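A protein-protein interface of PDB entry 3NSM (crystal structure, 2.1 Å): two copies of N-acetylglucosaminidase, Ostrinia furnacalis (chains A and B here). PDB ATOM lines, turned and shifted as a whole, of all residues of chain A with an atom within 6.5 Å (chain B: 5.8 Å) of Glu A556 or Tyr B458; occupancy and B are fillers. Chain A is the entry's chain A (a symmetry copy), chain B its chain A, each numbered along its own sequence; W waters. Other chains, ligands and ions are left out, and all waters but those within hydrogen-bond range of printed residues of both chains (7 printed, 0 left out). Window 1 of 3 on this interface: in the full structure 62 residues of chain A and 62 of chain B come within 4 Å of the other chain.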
ATOM      1  N   TYR A 458      26.790 -20.871  -4.336  1.00  0.00           N
ATOM      2  CA  TYR A 458      25.351 -20.584  -4.445  1.00  0.00           C
ATOM      3  C   TYR A 458      24.859 -20.530  -5.892  1.00  0.00           C
ATOM      4  O   TYR A 458      25.619 -20.830  -6.810  1.00  0.00           O
ATOM      5  CB  TYR A 458      25.016 -19.309  -3.671  1.00  0.00           C
ATOM      6  CG  TYR A 458      25.351 -19.472  -2.218  1.00  0.00           C
ATOM      7  CD1 TYR A 458      24.395 -19.930  -1.317  1.00  0.00           C
ATOM      8  CD2 TYR A 458      26.636 -19.222  -1.750  1.00  0.00           C
ATOM      9  CE1 TYR A 458      24.703 -20.109   0.018  1.00  0.00           C
ATOM     10  CE2 TYR A 458      26.957 -19.401  -0.419  1.00  0.00           C
ATOM     11  CZ  TYR A 458      25.982 -19.847   0.449  1.00  0.00           C
ATOM     12  OH  TYR A 458      26.284 -20.020   1.772  1.00  0.00           O
ATOM     13  N   TYR A 472      30.675 -24.926  -2.959  1.00  0.00           N
ATOM     14  CA  TYR A 472      30.798 -24.282  -1.649  1.00  0.00           C
ATOM     15  C   TYR A 472      31.990 -24.865  -0.886  1.00  0.00           C
ATOM     16  O   TYR A 472      32.188 -26.081  -0.864  1.00  0.00           O
ATOM     17  CB  TYR A 472      29.495 -24.500  -0.867  1.00  0.00           C
ATOM     18  CG  TYR A 472      29.428 -23.895   0.524  1.00  0.00           C
ATOM     19  CD1 TYR A 472      29.789 -24.639   1.647  1.00  0.00           C
ATOM     20  CD2 TYR A 472      28.963 -22.600   0.720  1.00  0.00           C
ATOM     21  CE1 TYR A 472      29.718 -24.096   2.932  1.00  0.00           C
ATOM     22  CE2 TYR A 472      28.885 -22.046   1.999  1.00  0.00           C
ATOM     23  CZ  TYR A 472      29.260 -22.802   3.097  1.00  0.00           C
ATOM     24  OH  TYR A 472      29.180 -22.270   4.360  1.00  0.00           O
ATOM     25  N   GLY A 474      33.801 -25.977   2.274  1.00  0.00           N
ATOM     26  CA  GLY A 474      33.573 -26.384   3.663  1.00  0.00           C
ATOM     27  C   GLY A 474      34.702 -25.919   4.551  1.00  0.00           C
ATOM     28  O   GLY A 474      35.784 -25.622   4.057  1.00  0.00           O
ATOM     29  N   ASP A 512      26.514 -13.247   8.661  1.00  0.00           N
ATOM     30  CA  ASP A 512      26.929 -14.137   9.726  1.00  0.00           C
ATOM     31  C   ASP A 512      27.191 -15.590   9.254  1.00  0.00           C
ATOM     32  O   ASP A 512      28.192 -16.187   9.578  1.00  0.00           O
ATOM     33  CB  ASP A 512      25.909 -14.192  10.849  1.00  0.00           C
ATOM     34  CG  ASP A 512      25.837 -12.950  11.690  1.00  0.00           C
ATOM     35  OD1 ASP A 512      26.562 -11.982  11.569  1.00  0.00           O
ATOM     36  OD2 ASP A 512      25.023 -12.985  12.550  1.00  0.00           O
ATOM     37  N   GLY A 513      26.280 -16.106   8.452  1.00  0.00           N
ATOM     38  CA  GLY A 513      26.407 -17.416   7.889  1.00  0.00           C
ATOM     39  C   GLY A 513      27.560 -17.579   6.946  1.00  0.00           C
ATOM     40  O   GLY A 513      28.224 -18.555   6.966  1.00  0.00           O
ATOM     41  N   ARG A 514      27.775 -16.586   6.109  1.00  0.00           N
ATOM     42  CA  ARG A 514      28.880 -16.608   5.145  1.00  0.00           C
ATOM     43  C   ARG A 514      30.238 -16.743   5.832  1.00  0.00           C
ATOM     44  O   ARG A 514      31.088 -17.536   5.405  1.00  0.00           O
ATOM     45  CB  ARG A 514      28.871 -15.355   4.268  1.00  0.00           C
ATOM     46  CG  ARG A 514      27.766 -15.312   3.202  1.00  0.00           C
ATOM     47  CD  ARG A 514      27.931 -16.411   2.169  1.00  0.00           C
ATOM     48  NE  ARG A 514      27.093 -16.201   0.974  1.00  0.00           N
ATOM     49  CZ  ARG A 514      25.801 -16.506   0.892  1.00  0.00           C
ATOM     50  NH1 ARG A 514      25.157 -17.018   1.935  1.00  0.00           N
ATOM     51  NH2 ARG A 514      25.141 -16.288  -0.246  1.00  0.00           N
ATOM     52  N   TRP A 516      30.920 -17.313   9.338  1.00  0.00           N
ATOM     53  CA  TRP A 516      31.051 -18.107  10.559  1.00  0.00           C
ATOM     54  C   TRP A 516      30.294 -19.422  10.453  1.00  0.00           C
ATOM     55  O   TRP A 516      29.146 -19.444  10.002  1.00  0.00           O
ATOM     56  CB  TRP A 516      30.591 -17.297  11.785  1.00  0.00           C
ATOM     57  CG  TRP A 516      31.151 -15.909  11.762  1.00  0.00           C
ATOM     58  CD1 TRP A 516      30.475 -14.749  11.497  1.00  0.00           C
ATOM     59  CD2 TRP A 516      32.520 -15.536  11.971  1.00  0.00           C
ATOM     60  NE1 TRP A 516      31.338 -13.680  11.529  1.00  0.00           N
ATOM     61  CE2 TRP A 516      32.599 -14.135  11.818  1.00  0.00           C
ATOM     62  CE3 TRP A 516      33.693 -16.256  12.264  1.00  0.00           C
ATOM     63  CZ2 TRP A 516      33.803 -13.430  11.955  1.00  0.00           C
ATOM     64  CZ3 TRP A 516      34.891 -15.553  12.407  1.00  0.00           C
ATOM     65  CH2 TRP A 516      34.933 -14.153  12.246  1.00  0.00           C
ATOM     66  N   PRO A 517      30.920 -20.525  10.897  1.00  0.00           N
ATOM     67  CA  PRO A 517      32.217 -20.588  11.577  1.00  0.00           C
ATOM     68  C   PRO A 517      33.460 -20.761  10.687  1.00  0.00           C
ATOM     69  O   PRO A 517      34.567 -20.908  11.220  1.00  0.00           O
ATOM     70  CB  PRO A 517      32.056 -21.822  12.464  1.00  0.00           C
ATOM     71  CG  PRO A 517      31.186 -22.726  11.662  1.00  0.00           C
ATOM     72  CD  PRO A 517      30.305 -21.860  10.793  1.00  0.00           C
ATOM     73  N   ARG A 518      33.285 -20.730   9.364  1.00  0.00           N
ATOM     74  CA  ARG A 518      34.390 -21.005   8.430  1.00  0.00           C
ATOM     75  C   ARG A 518      35.632 -20.140   8.626  1.00  0.00           C
ATOM     76  O   ARG A 518      36.759 -20.640   8.507  1.00  0.00           O
ATOM     77  CB  ARG A 518      33.921 -20.919   6.972  1.00  0.00           C
ATOM     78  CG  ARG A 518      33.083 -22.103   6.508  1.00  0.00           C
ATOM     79  CD  ARG A 518      32.812 -22.004   5.008  1.00  0.00           C
ATOM     80  NE  ARG A 518      32.065 -20.790   4.662  1.00  0.00           N
ATOM     81  CZ  ARG A 518      31.831 -20.376   3.419  1.00  0.00           C
ATOM     82  NH1 ARG A 518      32.288 -21.071   2.383  1.00  0.00           N
ATOM     83  NH2 ARG A 518      31.140 -19.260   3.212  1.00  0.00           N
ATOM     84  N   ARG A 545      31.621 -23.002  17.019  1.00  0.00           N
ATOM     85  CA  ARG A 545      30.343 -22.676  16.380  1.00  0.00           C
ATOM     86  C   ARG A 545      29.265 -22.363  17.418  1.00  0.00           C
ATOM     87  O   ARG A 545      28.562 -21.355  17.308  1.00  0.00           O
ATOM     88  CB  ARG A 545      29.882 -23.814  15.457  1.00  0.00           C
ATOM     89  CG  ARG A 545      28.694 -23.461  14.549  1.00  0.00           C
ATOM     90  CD  ARG A 545      27.326 -23.690  15.209  1.00  0.00           C
ATOM     91  NE  ARG A 545      26.244 -23.237  14.330  1.00  0.00           N
ATOM     92  CZ  ARG A 545      24.947 -23.398  14.563  1.00  0.00           C
ATOM     93  NH1 ARG A 545      24.520 -24.009  15.661  1.00  0.00           N
ATOM     94  NH2 ARG A 545      24.069 -22.936  13.682  1.00  0.00           N
ATOM     95  N   VAL A 549      27.177 -18.729  18.187  1.00  0.00           N
ATOM     96  CA  VAL A 549      25.711 -18.680  18.319  1.00  0.00           C
ATOM     97  C   VAL A 549      25.315 -18.034  19.658  1.00  0.00           C
ATOM     98  O   VAL A 549      24.430 -17.178  19.703  1.00  0.00           O
ATOM     99  CB  VAL A 549      25.071 -20.080  18.173  1.00  0.00           C
ATOM    100  CG1 VAL A 549      23.600 -20.061  18.568  1.00  0.00           C
ATOM    101  CG2 VAL A 549      25.235 -20.599  16.746  1.00  0.00           C
ATOM    102  N   ILE A 553      25.632 -14.505  16.955  1.00  0.00           N
ATOM    103  CA  ILE A 553      26.015 -14.743  15.566  1.00  0.00           C
ATOM    104  C   ILE A 553      25.152 -15.867  14.981  1.00  0.00           C
ATOM    105  O   ILE A 553      25.035 -16.945  15.568  1.00  0.00           O
ATOM    106  CB  ILE A 553      27.523 -15.124  15.431  1.00  0.00           C
ATOM    107  CG1 ILE A 553      28.428 -14.124  16.175  1.00  0.00           C
ATOM    108  CG2 ILE A 553      27.933 -15.296  13.963  1.00  0.00           C
ATOM    109  CD1 ILE A 553      28.360 -12.696  15.681  1.00  0.00           C
ATOM    110  N   GLN A 554      24.541 -15.609  13.831  1.00  0.00           N
ATOM    111  CA  GLN A 554      23.759 -16.626  13.147  1.00  0.00           C
ATOM    112  C   GLN A 554      24.701 -17.491  12.313  1.00  0.00           C
ATOM    113  O   GLN A 554      24.652 -17.488  11.081  1.00  0.00           O
ATOM    114  CB  GLN A 554      22.682 -15.991  12.257  1.00  0.00           C
ATOM    115  CG  GLN A 554      21.854 -14.909  12.915  1.00  0.00           C
ATOM    116  CD  GLN A 554      21.072 -15.409  14.098  1.00  0.00           C
ATOM    117  OE1 GLN A 554      21.441 -15.148  15.242  1.00  0.00           O
ATOM    118  NE2 GLN A 554      19.989 -16.134  13.844  1.00  0.00           N
ATOM    119  N   ALA A 555      25.565 -18.230  13.001  1.00  0.00           N
ATOM    120  CA  ALA A 555      26.575 -19.033  12.345  1.00  0.00           C
ATOM    121  C   ALA A 555      25.947 -20.188  11.586  1.00  0.00           C
ATOM    122  O   ALA A 555      24.926 -20.739  12.006  1.00  0.00           O
ATOM    123  CB  ALA A 555      27.568 -19.565  13.375  1.00  0.00           C
ATOM    124  N   GLU A 556      26.581 -20.572  10.480  1.00  0.00           N
ATOM    125  CA  GLU A 556      26.232 -21.810   9.793  1.00  0.00           C
ATOM    126  C   GLU A 556      26.246 -22.998  10.744  1.00  0.00           C
ATOM    127  O   GLU A 556      26.966 -22.998  11.753  1.00  0.00           O
ATOM    128  CB  GLU A 556      27.192 -22.086   8.635  1.00  0.00           C
ATOM    129  CG  GLU A 556      26.704 -21.546   7.305  1.00  0.00           C
ATOM    130  CD  GLU A 556      25.381 -22.148   6.868  1.00  0.00           C
ATOM    131  OE1 GLU A 556      24.580 -21.421   6.239  1.00  0.00           O
ATOM    132  OE2 GLU A 556      25.139 -23.341   7.158  1.00  0.00           O
ATOM    133  N   SER A 557      25.434 -24.001  10.415  1.00  0.00           N
ATOM    134  CA  SER A 557      25.423 -25.262  11.130  1.00  0.00           C
ATOM    135  C   SER A 557      26.327 -26.259  10.407  1.00  0.00           C
ATOM    136  O   SER A 557      26.249 -26.407   9.181  1.00  0.00           O
ATOM    137  CB  SER A 557      24.011 -25.794  11.217  1.00  0.00           C
ATOM    138  OG  SER A 557      23.985 -27.045  11.861  1.00  0.00           O
ATOM    139  N   LEU A 558      27.188 -26.938  11.164  1.00  0.00           N
ATOM    140  CA  LEU A 558      28.143 -27.879  10.567  1.00  0.00           C
ATOM    141  C   LEU A 558      27.650 -29.321  10.579  1.00  0.00           C
ATOM    142  O   LEU A 558      27.831 -30.052   9.604  1.00  0.00           O
ATOM    143  CB  LEU A 558      29.486 -27.799  11.294  1.00  0.00           C
ATOM    144  CG  LEU A 558      30.586 -26.859  10.793  1.00  0.00           C
ATOM    145  CD1 LEU A 558      30.078 -25.696   9.968  1.00  0.00           C
ATOM    146  CD2 LEU A 558      31.457 -26.391  11.961  1.00  0.00           C
ATOM    147  N   PHE B 454      16.329 -28.403   0.034  1.00  0.00           N
ATOM    148  CA  PHE B 454      16.922 -27.094   0.331  1.00  0.00           C
ATOM    149  C   PHE B 454      18.172 -27.180   1.202  1.00  0.00           C
ATOM    150  O   PHE B 454      18.815 -26.167   1.471  1.00  0.00           O
ATOM    151  CB  PHE B 454      15.876 -26.174   0.974  1.00  0.00           C
ATOM    152  CG  PHE B 454      14.940 -25.529  -0.015  1.00  0.00           C
ATOM    153  CD1 PHE B 454      14.771 -26.058  -1.299  1.00  0.00           C
ATOM    154  CD2 PHE B 454      14.208 -24.406   0.339  1.00  0.00           C
ATOM    155  CE1 PHE B 454      13.903 -25.460  -2.204  1.00  0.00           C
ATOM    156  CE2 PHE B 454      13.339 -23.809  -0.563  1.00  0.00           C
ATOM    157  CZ  PHE B 454      13.190 -24.336  -1.838  1.00  0.00           C
ATOM    158  N   ASP B 455      18.517 -28.396   1.613  1.00  0.00           N
ATOM    159  CA  ASP B 455      19.695 -28.654   2.428  1.00  0.00           C
ATOM    160  C   ASP B 455      20.966 -28.876   1.593  1.00  0.00           C
ATOM    161  O   ASP B 455      22.091 -28.726   2.108  1.00  0.00           O
ATOM    162  CB  ASP B 455      19.436 -29.851   3.352  1.00  0.00           C
ATOM    163  CG  ASP B 455      19.064 -31.124   2.596  1.00  0.00           C
ATOM    164  OD1 ASP B 455      18.201 -31.073   1.685  1.00  0.00           O
ATOM    165  OD2 ASP B 455      19.629 -32.191   2.931  1.00  0.00           O
ATOM    166  N   CYS B 456      20.783 -29.220   0.313  1.00  0.00           N
ATOM    167  CA  CYS B 456      21.889 -29.551  -0.596  1.00  0.00           C
ATOM    168  C   CYS B 456      22.871 -28.411  -0.833  1.00  0.00           C
ATOM    169  O   CYS B 456      22.477 -27.250  -0.917  1.00  0.00           O
ATOM    170  CB  CYS B 456      21.359 -29.975  -1.975  1.00  0.00           C
ATOM    171  SG  CYS B 456      20.136 -31.279  -1.981  1.00  0.00           S
ATOM    172  N   GLY B 457      24.150 -28.760  -0.973  1.00  0.00           N
ATOM    173  CA  GLY B 457      25.141 -27.812  -1.454  1.00  0.00           C
ATOM    174  C   GLY B 457      26.283 -27.462  -0.523  1.00  0.00           C
ATOM    175  O   GLY B 457      27.326 -26.997  -0.982  1.00  0.00           O
ATOM    176  N   TYR B 458      26.103 -27.685   0.775  1.00  0.00           N
ATOM    177  CA  TYR B 458      27.098 -27.260   1.772  1.00  0.00           C
ATOM    178  C   TYR B 458      28.202 -28.294   1.994  1.00  0.00           C
ATOM    179  O   TYR B 458      28.255 -29.297   1.285  1.00  0.00           O
ATOM    180  CB  TYR B 458      26.396 -26.873   3.073  1.00  0.00           C
ATOM    181  CG  TYR B 458      25.450 -25.732   2.842  1.00  0.00           C
ATOM    182  CD1 TYR B 458      25.871 -24.417   3.012  1.00  0.00           C
ATOM    183  CD2 TYR B 458      24.151 -25.961   2.402  1.00  0.00           C
ATOM    184  CE1 TYR B 458      25.014 -23.359   2.775  1.00  0.00           C
ATOM    185  CE2 TYR B 458      23.287 -24.912   2.158  1.00  0.00           C
ATOM    186  CZ  TYR B 458      23.734 -23.620   2.346  1.00  0.00           C
ATOM    187  OH  TYR B 458      22.886 -22.571   2.116  1.00  0.00           O
ATOM    188  N   GLY B 459      29.088 -28.039   2.959  1.00  0.00           N
ATOM    189  CA  GLY B 459      30.205 -28.949   3.238  1.00  0.00           C
ATOM    190  C   GLY B 459      29.712 -30.294   3.731  1.00  0.00           C
ATOM    191  O   GLY B 459      28.572 -30.414   4.184  1.00  0.00           O
ATOM    192  N   ALA B 460      30.558 -31.318   3.626  1.00  0.00           N
ATOM    193  CA  ALA B 460      30.250 -32.618   4.219  1.00  0.00           C
ATOM    194  C   ALA B 460      30.064 -32.447   5.722  1.00  0.00           C
ATOM    195  O   ALA B 460      30.724 -31.607   6.331  1.00  0.00           O
ATOM    196  CB  ALA B 460      31.367 -33.596   3.943  1.00  0.00           C
ATOM    197  N   GLY B 465      34.683 -32.648   1.855  1.00  0.00           N
ATOM    198  CA  GLY B 465      34.020 -32.424   0.575  1.00  0.00           C
ATOM    199  C   GLY B 465      32.705 -31.687   0.767  1.00  0.00           C
ATOM    200  O   GLY B 465      32.600 -30.795   1.618  1.00  0.00           O
ATOM    201  N   ASN B 466      31.706 -32.058  -0.026  1.00  0.00           N
ATOM    202  CA  ASN B 466      30.381 -31.448   0.047  1.00  0.00           C
ATOM    203  C   ASN B 466      29.325 -32.479   0.419  1.00  0.00           C
ATOM    204  O   ASN B 466      29.573 -33.682   0.316  1.00  0.00           O
ATOM    205  CB  ASN B 466      30.025 -30.768  -1.286  1.00  0.00           C
ATOM    206  CG  ASN B 466      30.859 -29.520  -1.549  1.00  0.00           C
ATOM    207  OD1 ASN B 466      31.847 -29.568  -2.279  1.00  0.00           O
ATOM    208  ND2 ASN B 466      30.470 -28.401  -0.945  1.00  0.00           N
ATOM    209  N   ASN B 467      28.145 -32.026   0.852  1.00  0.00           N
ATOM    210  CA  ASN B 467      27.106 -32.976   1.256  1.00  0.00           C
ATOM    211  C   ASN B 467      26.527 -33.750   0.064  1.00  0.00           C
ATOM    212  O   ASN B 467      26.751 -33.370  -1.089  1.00  0.00           O
ATOM    213  CB  ASN B 467      26.033 -32.321   2.144  1.00  0.00           C
ATOM    214  CG  ASN B 467      25.148 -31.334   1.399  1.00  0.00           C
ATOM    215  OD1 ASN B 467      24.852 -31.492   0.206  1.00  0.00           O
ATOM    216  ND2 ASN B 467      24.686 -30.319   2.123  1.00  0.00           N
ATOM    217  N   SER B 470      24.590 -32.255  -3.214  1.00  0.00           N
ATOM    218  CA  SER B 470      25.197 -31.096  -3.873  1.00  0.00           C
ATOM    219  C   SER B 470      25.131 -31.265  -5.401  1.00  0.00           C
ATOM    220  O   SER B 470      25.143 -32.403  -5.890  1.00  0.00           O
ATOM    221  CB  SER B 470      26.646 -30.923  -3.425  1.00  0.00           C
ATOM    222  OG  SER B 470      26.723 -30.706  -2.022  1.00  0.00           O
ATOM    223  N   TYR B 472      24.232 -26.856  -4.634  1.00  0.00           N
ATOM    224  CA  TYR B 472      23.177 -26.006  -4.077  1.00  0.00           C
ATOM    225  C   TYR B 472      22.143 -25.677  -5.157  1.00  0.00           C
ATOM    226  O   TYR B 472      22.500 -25.351  -6.290  1.00  0.00           O
ATOM    227  CB  TYR B 472      23.814 -24.723  -3.528  1.00  0.00           C
ATOM    228  CG  TYR B 472      22.872 -23.711  -2.899  1.00  0.00           C
ATOM    229  CD1 TYR B 472      22.328 -22.673  -3.656  1.00  0.00           C
ATOM    230  CD2 TYR B 472      22.562 -23.766  -1.546  1.00  0.00           C
ATOM    231  CE1 TYR B 472      21.471 -21.730  -3.084  1.00  0.00           C
ATOM    232  CE2 TYR B 472      21.709 -22.828  -0.961  1.00  0.00           C
ATOM    233  CZ  TYR B 472      21.173 -21.813  -1.736  1.00  0.00           C
ATOM    234  OH  TYR B 472      20.339 -20.881  -1.170  1.00  0.00           O
ATOM    235  N   GLN B 505      22.477 -30.016   8.859  1.00  0.00           N
ATOM    236  CA  GLN B 505      23.306 -28.831   8.737  1.00  0.00           C
ATOM    237  C   GLN B 505      22.469 -27.555   8.697  1.00  0.00           C
ATOM    238  O   GLN B 505      22.808 -26.606   7.988  1.00  0.00           O
ATOM    239  CB  GLN B 505      24.149 -28.916   7.465  1.00  0.00           C
ATOM    240  CG  GLN B 505      25.124 -30.072   7.446  1.00  0.00           C
ATOM    241  CD  GLN B 505      25.951 -30.078   6.195  1.00  0.00           C
ATOM    242  OE1 GLN B 505      27.082 -29.608   6.202  1.00  0.00           O
ATOM    243  NE2 GLN B 505      25.392 -30.598   5.105  1.00  0.00           N
ATOM    244  N   SER B 509      19.574 -20.787  13.485  1.00  0.00           N
ATOM    245  CA  SER B 509      20.395 -19.706  12.939  1.00  0.00           C
ATOM    246  C   SER B 509      20.379 -19.613  11.422  1.00  0.00           C
ATOM    247  O   SER B 509      20.658 -18.549  10.878  1.00  0.00           O
ATOM    248  CB  SER B 509      21.851 -19.851  13.408  1.00  0.00           C
ATOM    249  OG  SER B 509      21.938 -19.701  14.813  1.00  0.00           O
ATOM    250  N   THR B 510      20.088 -20.699  10.740  1.00  0.00           N
ATOM    251  CA  THR B 510      20.208 -20.799   9.293  1.00  0.00           C
ATOM    252  C   THR B 510      18.880 -20.951   8.576  1.00  0.00           C
ATOM    253  O   THR B 510      18.775 -21.006   7.397  1.00  0.00           O
ATOM    254  CB  THR B 510      21.054 -21.991   8.926  1.00  0.00           C
ATOM    255  OG1 THR B 510      20.408 -23.148   9.374  1.00  0.00           O
ATOM    256  CG2 THR B 510      22.432 -21.911   9.554  1.00  0.00           C
ATOM    257  N   GLY B 513      17.701 -18.174   5.820  1.00  0.00           N
ATOM    258  CA  GLY B 513      18.459 -18.282   4.611  1.00  0.00           C
ATOM    259  C   GLY B 513      18.178 -19.517   3.809  1.00  0.00           C
ATOM    260  O   GLY B 513      18.093 -19.466   2.632  1.00  0.00           O
ATOM    261  N   ARG B 514      18.043 -20.637   4.487  1.00  0.00           N
ATOM    262  CA  ARG B 514      17.749 -21.913   3.828  1.00  0.00           C
ATOM    263  C   ARG B 514      16.443 -21.862   3.036  1.00  0.00           C
ATOM    264  O   ARG B 514      16.379 -22.329   1.890  1.00  0.00           O
ATOM    265  CB  ARG B 514      17.688 -23.056   4.844  1.00  0.00           C
ATOM    266  CG  ARG B 514      19.047 -23.504   5.402  1.00  0.00           C
ATOM    267  CD  ARG B 514      19.937 -24.095   4.325  1.00  0.00           C
ATOM    268  NE  ARG B 514      21.096 -24.820   4.877  1.00  0.00           N
ATOM    269  CZ  ARG B 514      22.219 -24.245   5.297  1.00  0.00           C
ATOM    270  NH1 ARG B 514      22.358 -22.924   5.264  1.00  0.00           N
ATOM    271  NH2 ARG B 514      23.215 -24.999   5.764  1.00  0.00           N
ATOM    272  N   ARG B 518      14.021 -18.877  -1.747  1.00  0.00           N
ATOM    273  CA  ARG B 518      13.819 -20.047  -2.618  1.00  0.00           C
ATOM    274  C   ARG B 518      12.435 -20.685  -2.530  1.00  0.00           C
ATOM    275  O   ARG B 518      11.880 -21.102  -3.557  1.00  0.00           O
ATOM    276  CB  ARG B 518      14.898 -21.110  -2.381  1.00  0.00           C
ATOM    277  CG  ARG B 518      16.261 -20.768  -2.968  1.00  0.00           C
ATOM    278  CD  ARG B 518      17.212 -21.955  -2.828  1.00  0.00           C
ATOM    279  NE  ARG B 518      17.430 -22.323  -1.425  1.00  0.00           N
ATOM    280  CZ  ARG B 518      18.084 -23.410  -1.023  1.00  0.00           C
ATOM    281  NH1 ARG B 518      18.590 -24.257  -1.913  1.00  0.00           N
ATOM    282  NH2 ARG B 518      18.230 -23.652   0.276  1.00  0.00           N
ATOM    283  N   GLU B 556      18.296 -15.146   1.996  1.00  0.00           N
ATOM    284  CA  GLU B 556      19.441 -15.181   1.093  1.00  0.00           C
ATOM    285  C   GLU B 556      19.431 -13.999   0.134  1.00  0.00           C
ATOM    286  O   GLU B 556      18.368 -13.449  -0.188  1.00  0.00           O
ATOM    287  CB  GLU B 556      19.464 -16.479   0.284  1.00  0.00           C
ATOM    288  CG  GLU B 556      20.297 -17.573   0.923  1.00  0.00           C
ATOM    289  CD  GLU B 556      21.757 -17.189   1.087  1.00  0.00           C
ATOM    290  OE1 GLU B 556      22.371 -17.617   2.089  1.00  0.00           O
ATOM    291  OE2 GLU B 556      22.286 -16.456   0.222  1.00  0.00           O
HETATM  292  O   HOH W   1      28.491 -26.863  -3.226  1.00  0.00           O
HETATM  293  O   HOH W   2      30.202 -29.794   8.317  1.00  0.00           O
HETATM  294  O   HOH W   3      22.695 -17.588   9.034  1.00  0.00           O
HETATM  295  O   HOH W   4      34.623 -28.596   1.205  1.00  0.00           O
HETATM  296  O   HOH W   5      20.677 -18.071  16.339  1.00  0.00           O
HETATM  297  O   HOH W   6      19.022 -15.901  11.448  1.00  0.00           O
HETATM  298  O   HOH W   7      34.099 -27.997  -1.407  1.00  0.00           O
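The guanidinium group (NH1) of Arg B514 lies within salt-bridge range of the side-chain carboxylate (OE1) of Glu A556.
NH1 of Arg A514 is in salt-bridge range of OE1 of Glu B556.
ND2 of Asn B466 is in hydrogen-bond range of O of Tyr A472, at 2.9 Å.
The side-chain hydroxyl of Tyr B472 is in hydrogen-bond range of the guanidinium group of Arg B518, at 3.3 Å.
O of Gln B505 lies within hydrogen-bond range of NH2 of Arg B514 (2.8 Å).
The backbone NH (N) of Gly B457 sits at hydrogen-bond distance from the side-chain amide oxygen (OD1) of Asn B467, at 3.1 Å.
NH1 of Arg A514 sits at hydrogen-bond distance from OH of Tyr A458 (3.2 Å).
The side-chain hydroxyl of Tyr B458 lies within hydrogen-bond range of the guanidinium group of Arg B514, 3.2 Å away.
The backbone carbonyl oxygen of Tyr B458 sits at hydrogen-bond distance from the backbone NH of Asn B467, at 2.8 Å.
Among the printed residues, merely in contact across the chains: Tyr A472 with Gly B457 (3.3 Å), Ser A557 with Gln B505 (3.4 Å), Leu A558 with Gln B505 (3.5 Å), Ala A555 with Ser B509 (3.5 Å), Gln A554 with Ser B509 (3.5 Å), Ala A555 with Thr B510 (3.7 Å), Tyr A458 with Tyr B458 (3.7 Å), Tyr A472 with Gly B459 (3.7 Å), Tyr A472 with Tyr B458 (3.8 Å), Tyr A458 with Tyr B472 (3.8 Å), Ser A557 with Thr B510 (3.8 Å), Glu A556 with Thr B510 (3.8 Å), Arg A545 with Ser B509 (3.8 Å), Val A549 with Ser B509 (3.9 Å), Tyr A458 with Glu B556 (3.99 Å) and Glu A556 with Tyr B458 (3.99 Å).
Of the printed residues of chain A, Tyr B458 touches Tyr A458 (3.7 Å), Tyr A472 (3.8 Å) and Glu A556 (3.99 Å).
Of the printed residues of chain B, Tyr A458 touches Tyr B458, Tyr B472 and Glu B556.
Of the printed residues of chain A, Ser B509 touches Arg A545 (3.8 Å), Val A549 (3.9 Å), Gln A554 (3.5 Å) and Ala A555 (3.5 Å).
Of the printed residues of chain A, Arg B514 touches Glu A556.
The nearest printed residue of chain A that does not touch Tyr B458 is Gly A474 (5.9 Å).
Hydrophobic or aromatic side chains of chain B within 4 Å of the printed part of chain A: Tyr B458 and Tyr B472.
Of the 17 printed residues of chain A, 10 touch a printed residue of chain B.
Printed residues of chain A that touch a printed residue of chain B: Tyr A458, Tyr A472, Arg A514, Arg A545, Val A549, Gln A554, Ala A555, Glu A556, Ser A557 and Leu A558.
Among the printed residues, 19 pairs touch across the chains.
Among the printed residues, Asp or Glu carboxylates within 4 Å of a Lys or Arg side-chain nitrogen of the other chain: Arg A514 with Glu B556 and Glu A556 with Arg B514.
Tyr A458 touches its own counterpart, Tyr B458.
Tyr A458 touches Tyr B472, and with the chains exchanged Tyr A472 touches Tyr B458.
Tyr A458 touches Glu B556, and with the chains exchanged Glu A556 touches Tyr B458.
Arg A514 touches Glu B556, and with the chains exchanged Glu A556 touches Arg B514.
Positions printed for both chains: 458, 472, 513, 514, 518 and 556.
Of the 19 pairs that touch across the chains among the printed residues, 7 have their exchanged pair printed and touching as well.
Water W1 lies within hydrogen-bond range of the backbone carbonyl oxygen of Gly B457 (2.5 Å), the backbone NH of Tyr A472 (2.9 Å) and the side-chain amide nitrogen of Asn B466 (3.4 Å).
Water W5 bridges the side-chain hydroxyl (OG) of Ser B509 (2.6 Å) and the side-chain amide oxygen (OE1) of Gln A554 (3.2 Å).
Water W6 bridges the side-chain amide nitrogen of Gln A554 (2.6 Å) and the backbone carbonyl oxygen of Ser B509 (3.2 Å).
Water W2 lies within hydrogen-bond range of the backbone carbonyl oxygen (O) of Leu A558 (2.7 Å) and the backbone carbonyl oxygen (O) of Ala B460 (2.7 Å).
Water W3 bridges O of Gln A554 and O of Ser B509.
Water W4 bridges the backbone NH (N) of Gly A474 (2.9 Å) and the backbone carbonyl oxygen (O) of Gly B465 (3.0 Å).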
